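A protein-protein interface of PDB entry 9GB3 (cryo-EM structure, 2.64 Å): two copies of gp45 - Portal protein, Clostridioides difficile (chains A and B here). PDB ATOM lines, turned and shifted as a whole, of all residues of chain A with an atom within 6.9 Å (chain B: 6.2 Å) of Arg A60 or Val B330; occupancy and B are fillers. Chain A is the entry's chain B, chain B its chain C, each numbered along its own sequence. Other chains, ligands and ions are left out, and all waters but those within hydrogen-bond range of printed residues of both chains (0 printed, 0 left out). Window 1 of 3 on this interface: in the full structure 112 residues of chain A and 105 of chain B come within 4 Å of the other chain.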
ATOM      1  N   LEU A  44     -17.801 -34.282 -29.648  1.00  0.00           N
ATOM      2  CA  LEU A  44     -17.304 -32.998 -29.164  1.00  0.00           C
ATOM      3  C   LEU A  44     -18.452 -32.056 -28.837  1.00  0.00           C
ATOM      4  O   LEU A  44     -18.400 -31.326 -27.840  1.00  0.00           O
ATOM      5  CB  LEU A  44     -16.384 -32.354 -30.202  1.00  0.00           C
ATOM      6  CG  LEU A  44     -15.047 -33.018 -30.529  1.00  0.00           C
ATOM      7  CD1 LEU A  44     -14.294 -32.199 -31.558  1.00  0.00           C
ATOM      8  CD2 LEU A  44     -14.205 -33.188 -29.295  1.00  0.00           C
ATOM      9  N   TYR A  45     -19.489 -32.046 -29.674  1.00  0.00           N
ATOM     10  CA  TYR A  45     -20.626 -31.168 -29.425  1.00  0.00           C
ATOM     11  C   TYR A  45     -21.318 -31.522 -28.118  1.00  0.00           C
ATOM     12  O   TYR A  45     -21.670 -30.635 -27.335  1.00  0.00           O
ATOM     13  CB  TYR A  45     -21.607 -31.247 -30.592  1.00  0.00           C
ATOM     14  CG  TYR A  45     -22.818 -30.360 -30.438  1.00  0.00           C
ATOM     15  CD1 TYR A  45     -22.745 -29.004 -30.714  1.00  0.00           C
ATOM     16  CD2 TYR A  45     -24.035 -30.880 -30.029  1.00  0.00           C
ATOM     17  CE1 TYR A  45     -23.846 -28.189 -30.579  1.00  0.00           C
ATOM     18  CE2 TYR A  45     -25.143 -30.072 -29.892  1.00  0.00           C
ATOM     19  CZ  TYR A  45     -25.043 -28.728 -30.170  1.00  0.00           C
ATOM     20  OH  TYR A  45     -26.145 -27.920 -30.034  1.00  0.00           O
ATOM     21  N   GLN A  46     -21.499 -32.811 -27.851  1.00  0.00           N
ATOM     22  CA  GLN A  46     -22.175 -33.265 -26.644  1.00  0.00           C
ATOM     23  C   GLN A  46     -21.230 -33.459 -25.465  1.00  0.00           C
ATOM     24  O   GLN A  46     -21.665 -33.953 -24.420  1.00  0.00           O
ATOM     25  CB  GLN A  46     -22.925 -34.572 -26.926  1.00  0.00           C
ATOM     26  CG  GLN A  46     -24.188 -34.768 -26.097  1.00  0.00           C
ATOM     27  CD  GLN A  46     -25.283 -33.777 -26.443  1.00  0.00           C
ATOM     28  OE1 GLN A  46     -25.253 -33.149 -27.500  1.00  0.00           O
ATOM     29  NE2 GLN A  46     -26.247 -33.622 -25.545  1.00  0.00           N
ATOM     30  N   ASN A  47     -19.956 -33.085 -25.597  1.00  0.00           N
ATOM     31  CA  ASN A  47     -18.993 -33.161 -24.503  1.00  0.00           C
ATOM     32  C   ASN A  47     -18.758 -34.600 -24.051  1.00  0.00           C
ATOM     33  O   ASN A  47     -18.457 -34.849 -22.883  1.00  0.00           O
ATOM     34  CB  ASN A  47     -19.448 -32.293 -23.321  1.00  0.00           C
ATOM     35  CG  ASN A  47     -18.304 -31.566 -22.637  1.00  0.00           C
ATOM     36  OD1 ASN A  47     -17.334 -31.157 -23.273  1.00  0.00           O
ATOM     37  ND2 ASN A  47     -18.420 -31.394 -21.329  1.00  0.00           N
ATOM     38  N   LYS A  53     -13.178 -33.783 -22.830  1.00  0.00           N
ATOM     39  CA  LYS A  53     -14.265 -33.424 -21.921  1.00  0.00           C
ATOM     40  C   LYS A  53     -14.021 -32.071 -21.264  1.00  0.00           C
ATOM     41  O   LYS A  53     -14.934 -31.244 -21.157  1.00  0.00           O
ATOM     42  CB  LYS A  53     -14.440 -34.509 -20.857  1.00  0.00           C
ATOM     43  CG  LYS A  53     -15.492 -35.546 -21.203  1.00  0.00           C
ATOM     44  CD  LYS A  53     -15.399 -36.760 -20.298  1.00  0.00           C
ATOM     45  CE  LYS A  53     -16.319 -37.875 -20.763  1.00  0.00           C
ATOM     46  NZ  LYS A  53     -17.743 -37.449 -20.826  1.00  0.00           N
ATOM     47  N   SER A  56     -13.721 -29.474 -24.709  1.00  0.00           N
ATOM     48  CA  SER A  56     -14.842 -29.321 -25.640  1.00  0.00           C
ATOM     49  C   SER A  56     -16.014 -28.549 -25.049  1.00  0.00           C
ATOM     50  O   SER A  56     -17.088 -28.526 -25.661  1.00  0.00           O
ATOM     51  CB  SER A  56     -15.314 -30.697 -26.111  1.00  0.00           C
ATOM     52  OG  SER A  56     -15.522 -31.567 -25.015  1.00  0.00           O
ATOM     53  N   SER A  57     -15.867 -27.917 -23.885  1.00  0.00           N
ATOM     54  CA  SER A  57     -16.938 -27.097 -23.339  1.00  0.00           C
ATOM     55  C   SER A  57     -17.276 -25.911 -24.230  1.00  0.00           C
ATOM     56  O   SER A  57     -18.407 -25.416 -24.180  1.00  0.00           O
ATOM     57  CB  SER A  57     -16.540 -26.609 -21.945  1.00  0.00           C
ATOM     58  OG  SER A  57     -16.411 -27.698 -21.050  1.00  0.00           O
ATOM     59  N   PHE A  58     -16.330 -25.448 -25.046  1.00  0.00           N
ATOM     60  CA  PHE A  58     -16.554 -24.282 -25.889  1.00  0.00           C
ATOM     61  C   PHE A  58     -17.322 -24.602 -27.163  1.00  0.00           C
ATOM     62  O   PHE A  58     -17.779 -23.672 -27.836  1.00  0.00           O
ATOM     63  CB  PHE A  58     -15.214 -23.648 -26.256  1.00  0.00           C
ATOM     64  CG  PHE A  58     -14.381 -23.267 -25.071  1.00  0.00           C
ATOM     65  CD1 PHE A  58     -14.605 -22.077 -24.407  1.00  0.00           C
ATOM     66  CD2 PHE A  58     -13.378 -24.103 -24.619  1.00  0.00           C
ATOM     67  CE1 PHE A  58     -13.842 -21.728 -23.315  1.00  0.00           C
ATOM     68  CE2 PHE A  58     -12.613 -23.757 -23.530  1.00  0.00           C
ATOM     69  CZ  PHE A  58     -12.844 -22.567 -22.877  1.00  0.00           C
ATOM     70  N   VAL A  59     -17.475 -25.880 -27.514  1.00  0.00           N
ATOM     71  CA  VAL A  59     -18.081 -26.232 -28.797  1.00  0.00           C
ATOM     72  C   VAL A  59     -19.549 -25.827 -28.828  1.00  0.00           C
ATOM     73  O   VAL A  59     -20.021 -25.229 -29.800  1.00  0.00           O
ATOM     74  CB  VAL A  59     -17.911 -27.736 -29.078  1.00  0.00           C
ATOM     75  CG1 VAL A  59     -18.652 -28.121 -30.360  1.00  0.00           C
ATOM     76  CG2 VAL A  59     -16.430 -28.105 -29.157  1.00  0.00           C
ATOM     77  N   ARG A  60     -20.295 -26.165 -27.776  1.00  0.00           N
ATOM     78  CA  ARG A  60     -21.727 -25.876 -27.759  1.00  0.00           C
ATOM     79  C   ARG A  60     -22.039 -24.392 -27.878  1.00  0.00           C
ATOM     80  O   ARG A  60     -22.867 -24.033 -28.733  1.00  0.00           O
ATOM     81  CB  ARG A  60     -22.357 -26.453 -26.487  1.00  0.00           C
ATOM     82  CG  ARG A  60     -22.537 -27.951 -26.510  1.00  0.00           C
ATOM     83  CD  ARG A  60     -23.600 -28.398 -25.529  1.00  0.00           C
ATOM     84  NE  ARG A  60     -24.947 -28.099 -26.009  1.00  0.00           N
ATOM     85  CZ  ARG A  60     -25.806 -28.972 -26.522  1.00  0.00           C
ATOM     86  NH1 ARG A  60     -25.501 -30.251 -26.682  1.00  0.00           N
ATOM     87  NH2 ARG A  60     -27.011 -28.549 -26.890  1.00  0.00           N
ATOM     88  N   PRO A  61     -21.460 -23.490 -27.073  1.00  0.00           N
ATOM     89  CA  PRO A  61     -21.817 -22.070 -27.226  1.00  0.00           C
ATOM     90  C   PRO A  61     -21.496 -21.505 -28.597  1.00  0.00           C
ATOM     91  O   PRO A  61     -22.305 -20.748 -29.137  1.00  0.00           O
ATOM     92  CB  PRO A  61     -21.011 -21.377 -26.116  1.00  0.00           C
ATOM     93  CG  PRO A  61     -20.012 -22.357 -25.671  1.00  0.00           C
ATOM     94  CD  PRO A  61     -20.596 -23.700 -25.900  1.00  0.00           C
ATOM     95  N   ILE A  62     -20.370 -21.896 -29.197  1.00  0.00           N
ATOM     96  CA  ILE A  62     -20.000 -21.383 -30.515  1.00  0.00           C
ATOM     97  C   ILE A  62     -21.065 -21.753 -31.543  1.00  0.00           C
ATOM     98  O   ILE A  62     -21.691 -20.884 -32.166  1.00  0.00           O
ATOM     99  CB  ILE A  62     -18.616 -21.919 -30.926  1.00  0.00           C
ATOM    100  CG1 ILE A  62     -17.518 -21.272 -30.080  1.00  0.00           C
ATOM    101  CG2 ILE A  62     -18.349 -21.678 -32.409  1.00  0.00           C
ATOM    102  CD1 ILE A  62     -16.232 -22.067 -30.022  1.00  0.00           C
ATOM    103  N   VAL A  63     -21.295 -23.058 -31.709  1.00  0.00           N
ATOM    104  CA  VAL A  63     -22.218 -23.545 -32.729  1.00  0.00           C
ATOM    105  C   VAL A  63     -23.624 -23.029 -32.464  1.00  0.00           C
ATOM    106  O   VAL A  63     -24.323 -22.584 -33.382  1.00  0.00           O
ATOM    107  CB  VAL A  63     -22.187 -25.083 -32.782  1.00  0.00           C
ATOM    108  CG1 VAL A  63     -23.247 -25.605 -33.747  1.00  0.00           C
ATOM    109  CG2 VAL A  63     -20.795 -25.570 -33.173  1.00  0.00           C
ATOM    110  N   ASN A  64     -24.062 -23.076 -31.206  1.00  0.00           N
ATOM    111  CA  ASN A  64     -25.452 -22.750 -30.917  1.00  0.00           C
ATOM    112  C   ASN A  64     -25.706 -21.251 -31.014  1.00  0.00           C
ATOM    113  O   ASN A  64     -26.762 -20.837 -31.500  1.00  0.00           O
ATOM    114  CB  ASN A  64     -25.846 -23.293 -29.545  1.00  0.00           C
ATOM    115  CG  ASN A  64     -26.109 -24.792 -29.566  1.00  0.00           C
ATOM    116  OD1 ASN A  64     -26.189 -25.405 -30.629  1.00  0.00           O
ATOM    117  ND2 ASN A  64     -26.253 -25.385 -28.392  1.00  0.00           N
ATOM    118  N   SER A  65     -24.756 -20.416 -30.589  1.00  0.00           N
ATOM    119  CA  SER A  65     -24.912 -18.982 -30.795  1.00  0.00           C
ATOM    120  C   SER A  65     -24.935 -18.647 -32.279  1.00  0.00           C
ATOM    121  O   SER A  65     -25.777 -17.858 -32.729  1.00  0.00           O
ATOM    122  CB  SER A  65     -23.786 -18.228 -30.091  1.00  0.00           C
ATOM    123  OG  SER A  65     -22.526 -18.566 -30.644  1.00  0.00           O
ATOM    124  N   THR A  66     -24.039 -19.256 -33.061  1.00  0.00           N
ATOM    125  CA  THR A  66     -23.995 -18.963 -34.489  1.00  0.00           C
ATOM    126  C   THR A  66     -25.290 -19.377 -35.177  1.00  0.00           C
ATOM    127  O   THR A  66     -25.834 -18.629 -35.997  1.00  0.00           O
ATOM    128  CB  THR A  66     -22.797 -19.663 -35.133  1.00  0.00           C
ATOM    129  OG1 THR A  66     -21.619 -19.416 -34.358  1.00  0.00           O
ATOM    130  CG2 THR A  66     -22.573 -19.155 -36.553  1.00  0.00           C
ATOM    131  N   LYS A 106     -22.273 -28.054 -37.058  1.00  0.00           N
ATOM    132  CA  LYS A 106     -21.634 -29.031 -36.181  1.00  0.00           C
ATOM    133  C   LYS A 106     -20.826 -30.054 -36.971  1.00  0.00           C
ATOM    134  O   LYS A 106     -19.675 -30.342 -36.626  1.00  0.00           O
ATOM    135  CB  LYS A 106     -22.702 -29.729 -35.340  1.00  0.00           C
ATOM    136  CG  LYS A 106     -22.176 -30.530 -34.163  1.00  0.00           C
ATOM    137  CD  LYS A 106     -23.089 -31.705 -33.817  1.00  0.00           C
ATOM    138  CE  LYS A 106     -24.527 -31.278 -33.533  1.00  0.00           C
ATOM    139  NZ  LYS A 106     -25.358 -32.432 -33.101  1.00  0.00           N
ATOM    140  N   PHE A 338     -19.095 -15.585 -24.267  1.00  0.00           N
ATOM    141  CA  PHE A 338     -18.237 -16.103 -23.208  1.00  0.00           C
ATOM    142  C   PHE A 338     -18.009 -15.045 -22.135  1.00  0.00           C
ATOM    143  O   PHE A 338     -16.905 -14.889 -21.612  1.00  0.00           O
ATOM    144  CB  PHE A 338     -16.907 -16.583 -23.780  1.00  0.00           C
ATOM    145  CG  PHE A 338     -17.045 -17.713 -24.755  1.00  0.00           C
ATOM    146  CD1 PHE A 338     -17.365 -18.984 -24.318  1.00  0.00           C
ATOM    147  CD2 PHE A 338     -16.859 -17.503 -26.109  1.00  0.00           C
ATOM    148  CE1 PHE A 338     -17.495 -20.024 -25.210  1.00  0.00           C
ATOM    149  CE2 PHE A 338     -16.986 -18.540 -27.006  1.00  0.00           C
ATOM    150  CZ  PHE A 338     -17.304 -19.802 -26.555  1.00  0.00           C
ATOM    151  N   GLU B 217     -33.252 -31.987 -27.580  1.00  0.00           N
ATOM    152  CA  GLU B 217     -31.980 -32.087 -28.293  1.00  0.00           C
ATOM    153  C   GLU B 217     -31.988 -33.273 -29.252  1.00  0.00           C
ATOM    154  O   GLU B 217     -31.041 -34.058 -29.324  1.00  0.00           O
ATOM    155  CB  GLU B 217     -30.807 -32.186 -27.314  1.00  0.00           C
ATOM    156  CG  GLU B 217     -30.632 -30.968 -26.421  1.00  0.00           C
ATOM    157  CD  GLU B 217     -30.138 -29.749 -27.174  1.00  0.00           C
ATOM    158  OE1 GLU B 217     -29.352 -29.912 -28.130  1.00  0.00           O
ATOM    159  OE2 GLU B 217     -30.535 -28.624 -26.808  1.00  0.00           O
ATOM    160  N   GLN B 226     -31.947 -36.201 -25.651  1.00  0.00           N
ATOM    161  CA  GLN B 226     -30.804 -35.995 -24.776  1.00  0.00           C
ATOM    162  C   GLN B 226     -31.166 -34.973 -23.710  1.00  0.00           C
ATOM    163  O   GLN B 226     -31.756 -33.932 -24.011  1.00  0.00           O
ATOM    164  CB  GLN B 226     -29.582 -35.512 -25.561  1.00  0.00           C
ATOM    165  CG  GLN B 226     -29.504 -36.040 -26.979  1.00  0.00           C
ATOM    166  CD  GLN B 226     -28.142 -35.830 -27.605  1.00  0.00           C
ATOM    167  OE1 GLN B 226     -27.173 -36.494 -27.241  1.00  0.00           O
ATOM    168  NE2 GLN B 226     -28.061 -34.907 -28.553  1.00  0.00           N
ATOM    169  N   ASP B 228     -30.467 -32.024 -20.948  1.00  0.00           N
ATOM    170  CA  ASP B 228     -29.560 -30.894 -20.810  1.00  0.00           C
ATOM    171  C   ASP B 228     -28.475 -31.138 -19.771  1.00  0.00           C
ATOM    172  O   ASP B 228     -27.496 -30.386 -19.736  1.00  0.00           O
ATOM    173  CB  ASP B 228     -30.345 -29.635 -20.440  1.00  0.00           C
ATOM    174  CG  ASP B 228     -30.968 -28.963 -21.643  1.00  0.00           C
ATOM    175  OD1 ASP B 228     -31.168 -29.644 -22.669  1.00  0.00           O
ATOM    176  OD2 ASP B 228     -31.257 -27.751 -21.562  1.00  0.00           O
ATOM    177  N   PRO B 231     -24.480 -32.873 -21.339  1.00  0.00           N
ATOM    178  CA  PRO B 231     -23.247 -32.138 -21.657  1.00  0.00           C
ATOM    179  C   PRO B 231     -22.459 -31.685 -20.438  1.00  0.00           C
ATOM    180  O   PRO B 231     -21.224 -31.648 -20.497  1.00  0.00           O
ATOM    181  CB  PRO B 231     -23.767 -30.944 -22.464  1.00  0.00           C
ATOM    182  CG  PRO B 231     -25.003 -31.425 -23.074  1.00  0.00           C
ATOM    183  CD  PRO B 231     -25.638 -32.277 -22.028  1.00  0.00           C
ATOM    184  N   ILE B 232     -23.132 -31.347 -19.336  1.00  0.00           N
ATOM    185  CA  ILE B 232     -22.457 -30.815 -18.152  1.00  0.00           C
ATOM    186  C   ILE B 232     -22.098 -31.889 -17.133  1.00  0.00           C
ATOM    187  O   ILE B 232     -21.343 -31.596 -16.194  1.00  0.00           O
ATOM    188  CB  ILE B 232     -23.301 -29.714 -17.467  1.00  0.00           C
ATOM    189  CG1 ILE B 232     -24.684 -30.233 -17.037  1.00  0.00           C
ATOM    190  CG2 ILE B 232     -23.453 -28.520 -18.396  1.00  0.00           C
ATOM    191  CD1 ILE B 232     -25.484 -29.238 -16.227  1.00  0.00           C
ATOM    192  N   LEU B 235     -18.530 -32.338 -16.105  1.00  0.00           N
ATOM    193  CA  LEU B 235     -18.124 -31.142 -15.378  1.00  0.00           C
ATOM    194  C   LEU B 235     -18.697 -31.135 -13.968  1.00  0.00           C
ATOM    195  O   LEU B 235     -18.019 -30.716 -13.025  1.00  0.00           O
ATOM    196  CB  LEU B 235     -18.552 -29.889 -16.139  1.00  0.00           C
ATOM    197  CG  LEU B 235     -18.041 -29.755 -17.574  1.00  0.00           C
ATOM    198  CD1 LEU B 235     -18.686 -28.561 -18.246  1.00  0.00           C
ATOM    199  CD2 LEU B 235     -16.528 -29.633 -17.604  1.00  0.00           C
ATOM    200  N   TYR B 325     -16.899 -21.889 -15.155  1.00  0.00           N
ATOM    201  CA  TYR B 325     -16.924 -21.278 -16.480  1.00  0.00           C
ATOM    202  C   TYR B 325     -17.275 -22.307 -17.543  1.00  0.00           C
ATOM    203  O   TYR B 325     -18.061 -22.025 -18.452  1.00  0.00           O
ATOM    204  CB  TYR B 325     -15.572 -20.633 -16.798  1.00  0.00           C
ATOM    205  CG  TYR B 325     -15.188 -19.416 -15.966  1.00  0.00           C
ATOM    206  CD1 TYR B 325     -16.091 -18.799 -15.106  1.00  0.00           C
ATOM    207  CD2 TYR B 325     -13.909 -18.885 -16.053  1.00  0.00           C
ATOM    208  CE1 TYR B 325     -15.728 -17.698 -14.363  1.00  0.00           C
ATOM    209  CE2 TYR B 325     -13.542 -17.785 -15.312  1.00  0.00           C
ATOM    210  CZ  TYR B 325     -14.455 -17.194 -14.471  1.00  0.00           C
ATOM    211  OH  TYR B 325     -14.094 -16.094 -13.728  1.00  0.00           O
ATOM    212  N   CYS B 326     -16.703 -23.507 -17.445  1.00  0.00           N
ATOM    213  CA  CYS B 326     -17.016 -24.554 -18.414  1.00  0.00           C
ATOM    214  C   CYS B 326     -18.486 -24.955 -18.342  1.00  0.00           C
ATOM    215  O   CYS B 326     -19.129 -25.176 -19.374  1.00  0.00           O
ATOM    216  CB  CYS B 326     -16.117 -25.767 -18.181  1.00  0.00           C
ATOM    217  SG  CYS B 326     -14.404 -25.526 -18.709  1.00  0.00           S
ATOM    218  N   ILE B 327     -19.033 -25.057 -17.128  1.00  0.00           N
ATOM    219  CA  ILE B 327     -20.438 -25.424 -16.967  1.00  0.00           C
ATOM    220  C   ILE B 327     -21.339 -24.348 -17.559  1.00  0.00           C
ATOM    221  O   ILE B 327     -22.331 -24.650 -18.233  1.00  0.00           O
ATOM    222  CB  ILE B 327     -20.761 -25.674 -15.481  1.00  0.00           C
ATOM    223  CG1 ILE B 327     -20.081 -26.954 -14.990  1.00  0.00           C
ATOM    224  CG2 ILE B 327     -22.267 -25.777 -15.261  1.00  0.00           C
ATOM    225  CD1 ILE B 327     -19.862 -27.000 -13.496  1.00  0.00           C
ATOM    226  N   VAL B 328     -21.016 -23.078 -17.308  1.00  0.00           N
ATOM    227  CA  VAL B 328     -21.828 -21.992 -17.846  1.00  0.00           C
ATOM    228  C   VAL B 328     -21.720 -21.946 -19.364  1.00  0.00           C
ATOM    229  O   VAL B 328     -22.702 -21.648 -20.053  1.00  0.00           O
ATOM    230  CB  VAL B 328     -21.417 -20.651 -17.207  1.00  0.00           C
ATOM    231  CG1 VAL B 328     -22.132 -19.478 -17.887  1.00  0.00           C
ATOM    232  CG2 VAL B 328     -21.694 -20.671 -15.705  1.00  0.00           C
ATOM    233  N   ASP B 329     -20.536 -22.226 -19.910  1.00  0.00           N
ATOM    234  CA  ASP B 329     -20.365 -22.224 -21.358  1.00  0.00           C
ATOM    235  C   ASP B 329     -21.167 -23.346 -22.004  1.00  0.00           C
ATOM    236  O   ASP B 329     -21.878 -23.123 -22.990  1.00  0.00           O
ATOM    237  CB  ASP B 329     -18.882 -22.356 -21.706  1.00  0.00           C
ATOM    238  CG  ASP B 329     -18.081 -21.119 -21.347  1.00  0.00           C
ATOM    239  OD1 ASP B 329     -18.685 -20.042 -21.169  1.00  0.00           O
ATOM    240  OD2 ASP B 329     -16.842 -21.223 -21.242  1.00  0.00           O
ATOM    241  N   VAL B 330     -21.075 -24.558 -21.451  1.00  0.00           N
ATOM    242  CA  VAL B 330     -21.737 -25.714 -22.052  1.00  0.00           C
ATOM    243  C   VAL B 330     -23.247 -25.525 -22.053  1.00  0.00           C
ATOM    244  O   VAL B 330     -23.914 -25.697 -23.079  1.00  0.00           O
ATOM    245  CB  VAL B 330     -21.338 -27.001 -21.306  1.00  0.00           C
ATOM    246  CG1 VAL B 330     -22.212 -28.153 -21.717  1.00  0.00           C
ATOM    247  CG2 VAL B 330     -19.917 -27.349 -21.595  1.00  0.00           C
ATOM    248  N   SER B 331     -23.810 -25.174 -20.898  1.00  0.00           N
ATOM    249  CA  SER B 331     -25.248 -24.977 -20.808  1.00  0.00           C
ATOM    250  C   SER B 331     -25.712 -23.732 -21.548  1.00  0.00           C
ATOM    251  O   SER B 331     -26.912 -23.600 -21.809  1.00  0.00           O
ATOM    252  CB  SER B 331     -25.671 -24.895 -19.343  1.00  0.00           C
ATOM    253  OG  SER B 331     -25.003 -23.840 -18.677  1.00  0.00           O
ATOM    254  N   GLU B 332     -24.798 -22.819 -21.884  1.00  0.00           N
ATOM    255  CA  GLU B 332     -25.135 -21.548 -22.525  1.00  0.00           C
ATOM    256  C   GLU B 332     -26.081 -20.722 -21.663  1.00  0.00           C
ATOM    257  O   GLU B 332     -26.868 -19.924 -22.174  1.00  0.00           O
ATOM    258  CB  GLU B 332     -25.737 -21.762 -23.914  1.00  0.00           C
ATOM    259  CG  GLU B 332     -24.809 -22.442 -24.883  1.00  0.00           C
ATOM    260  CD  GLU B 332     -25.541 -22.952 -26.092  1.00  0.00           C
ATOM    261  OE1 GLU B 332     -26.125 -22.129 -26.826  1.00  0.00           O
ATOM    262  OE2 GLU B 332     -25.541 -24.181 -26.303  1.00  0.00           O
ATOM    263  N   THR B 333     -26.008 -20.902 -20.356  1.00  0.00           N
ATOM    264  CA  THR B 333     -26.836 -20.118 -19.460  1.00  0.00           C
ATOM    265  C   THR B 333     -26.325 -18.680 -19.453  1.00  0.00           C
ATOM    266  O   THR B 333     -25.115 -18.467 -19.324  1.00  0.00           O
ATOM    267  CB  THR B 333     -26.795 -20.702 -18.051  1.00  0.00           C
ATOM    268  OG1 THR B 333     -26.900 -22.126 -18.124  1.00  0.00           O
ATOM    269  CG2 THR B 333     -27.943 -20.166 -17.216  1.00  0.00           C
ATOM    270  N   ARG B 362     -33.588 -20.802 -30.001  1.00  0.00           N
ATOM    271  CA  ARG B 362     -33.085 -22.092 -30.454  1.00  0.00           C
ATOM    272  C   ARG B 362     -33.785 -23.246 -29.746  1.00  0.00           C
ATOM    273  O   ARG B 362     -34.052 -24.281 -30.367  1.00  0.00           O
ATOM    274  CB  ARG B 362     -31.578 -22.170 -30.230  1.00  0.00           C
ATOM    275  CG  ARG B 362     -30.902 -23.336 -30.946  1.00  0.00           C
ATOM    276  CD  ARG B 362     -29.424 -23.442 -30.605  1.00  0.00           C
ATOM    277  NE  ARG B 362     -29.188 -23.513 -29.166  1.00  0.00           N
ATOM    278  CZ  ARG B 362     -29.478 -24.557 -28.400  1.00  0.00           C
ATOM    279  NH1 ARG B 362     -29.996 -25.668 -28.901  1.00  0.00           N
ATOM    280  NH2 ARG B 362     -29.237 -24.487 -27.094  1.00  0.00           N
ATOM    281  N   LYS B 363     -34.093 -23.090 -28.457  1.00  0.00           N
ATOM    282  CA  LYS B 363     -34.628 -24.207 -27.685  1.00  0.00           C
ATOM    283  C   LYS B 363     -36.086 -24.488 -28.031  1.00  0.00           C
ATOM    284  O   LYS B 363     -36.512 -25.647 -28.033  1.00  0.00           O
ATOM    285  CB  LYS B 363     -34.484 -23.929 -26.187  1.00  0.00           C
ATOM    286  CG  LYS B 363     -33.255 -24.557 -25.553  1.00  0.00           C
ATOM    287  CD  LYS B 363     -33.396 -26.065 -25.416  1.00  0.00           C
ATOM    288  CE  LYS B 363     -32.294 -26.645 -24.551  1.00  0.00           C
ATOM    289  NZ  LYS B 363     -32.154 -28.111 -24.752  1.00  0.00           N
ATOM    290  N   GLN B 366     -37.120 -27.137 -30.765  1.00  0.00           N
ATOM    291  CA  GLN B 366     -37.030 -28.571 -30.529  1.00  0.00           C
ATOM    292  C   GLN B 366     -38.359 -29.185 -30.110  1.00  0.00           C
ATOM    293  O   GLN B 366     -38.477 -30.415 -30.130  1.00  0.00           O
ATOM    294  CB  GLN B 366     -35.976 -28.860 -29.461  1.00  0.00           C
ATOM    295  CG  GLN B 366     -34.549 -28.713 -29.955  1.00  0.00           C
ATOM    296  CD  GLN B 366     -33.580 -28.385 -28.842  1.00  0.00           C
ATOM    297  OE1 GLN B 366     -33.756 -28.819 -27.706  1.00  0.00           O
ATOM    298  NE2 GLN B 366     -32.549 -27.614 -29.162  1.00  0.00           N
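No position is printed for both chains. Of the 17 pairs that touch across the chains among the printed residues, none has its exchanged pair printed and touching as well.
Of the 18 printed residues of chain A, 8 touch a printed residue of chain B. Printed residues of chain A that touch a printed residue of chain B: Gln A46, Asn A47, Ser A57, Phe A58, Arg A60, Pro A61, Asn A64 and Phe A338. Of the 18 printed residues of chain B, 9 touch a printed residue of chain A. Hydrophobic or aromatic side chains of chain B within 4 Å of the printed part of chain A: Pro B231, Leu B235 and Val B330.
O of Pro B231 lies within hydrogen-bond range of ND2 of Asn A47, 2.9 Å away. The guanidinium group of Arg B362 lies close to the side-chain amide nitrogen of Asn A64 (3.4 Å). The side-chain sulfur (SG) of Cys B326 sits close to the side-chain hydroxyl (OG) of Ser A57 (3.8 Å). The guanidinium group of Arg A60 lies within salt-bridge range of the side-chain carboxylate of Glu B332 (3.97 Å). The side-chain amide nitrogen (NE2) of Gln A46 sits close to the side-chain amide oxygen (OE1) of Gln B226 (3.5 Å). ND2 of Asn A64 sits at hydrogen-bond distance from OE2 of Glu B332. OE1 of Glu B217 lies within salt-bridge range of NH2 of Arg A60 (3.0 Å).
The guanidinium group of Arg B362 sits close to the side-chain amide nitrogen of Gln B366 (3.2 Å). The side-chain amide oxygen (OE1) of Gln A46 lies within hydrogen-bond range of the guanidinium group (NH1) of Arg A60. The backbone carbonyl oxygen (O) of Pro A61 is in hydrogen-bond range of the side-chain hydroxyl (OG) of Ser A65 (2.7 Å). The side-chain hydroxyl (OG) of Ser A56 sits at hydrogen-bond distance from the side-chain amide oxygen (OD1) of Asn A47. The guanidinium group of Arg B362 is in salt-bridge range of the side-chain carboxylate of Glu B332, 3.8 Å away. The side-chain carboxylate (OE2) of Glu B217 is in salt-bridge range of the side-chain amino group (NZ) of Lys B363 (2.7 Å).
Gln A46 touches Pro B231. Ser A57 touches Leu B235. Asp B329 touches Ser A57 (CB to O, 3.96 Å). Val B330 touches Ser A57. Phe A58 touches Asp B329 (CE1 to OD2, 3.7 Å). Arg A60 touches Pro B231. Val B330 touches Arg A60. Pro A61 touches Asp B329. Glu B332 touches Pro A61 (CG to CA, 3.8 Å). OD1 of Asp B329 touches CD1 of Phe A338 (3.6 Å).
Arg A60 touches just these residues of chain B: Glu B217 (3.0 Å), Pro B231 (3.8 Å), Val B330 (3.7 Å) and Glu B332 (3.6 Å). Of the printed residues of chain B, Phe A338 touches Asp B329 (3.6 Å). Printed residues of chain A within 4 Å of Glu B217: Arg A60 (3.0 Å). Printed residues of chain A within 4 Å of Gln B226: Gln A46 (3.4 Å). Printed residues of chain A within 4 Å of Pro B231: Gln A46 (3.5 Å), Asn A47 (2.9 Å) and Arg A60 (3.8 Å). Ile B327 touches none of the printed residues of chain A. Val B328 touches none of the printed residues of chain A. Of chain A, only Ser A57 (3.5 Å) and Arg A60 (3.7 Å) come within 4 Å of Val B330. The nearest residue of chain A that does not touch Val B330 is Asn A47 (4.3 Å).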
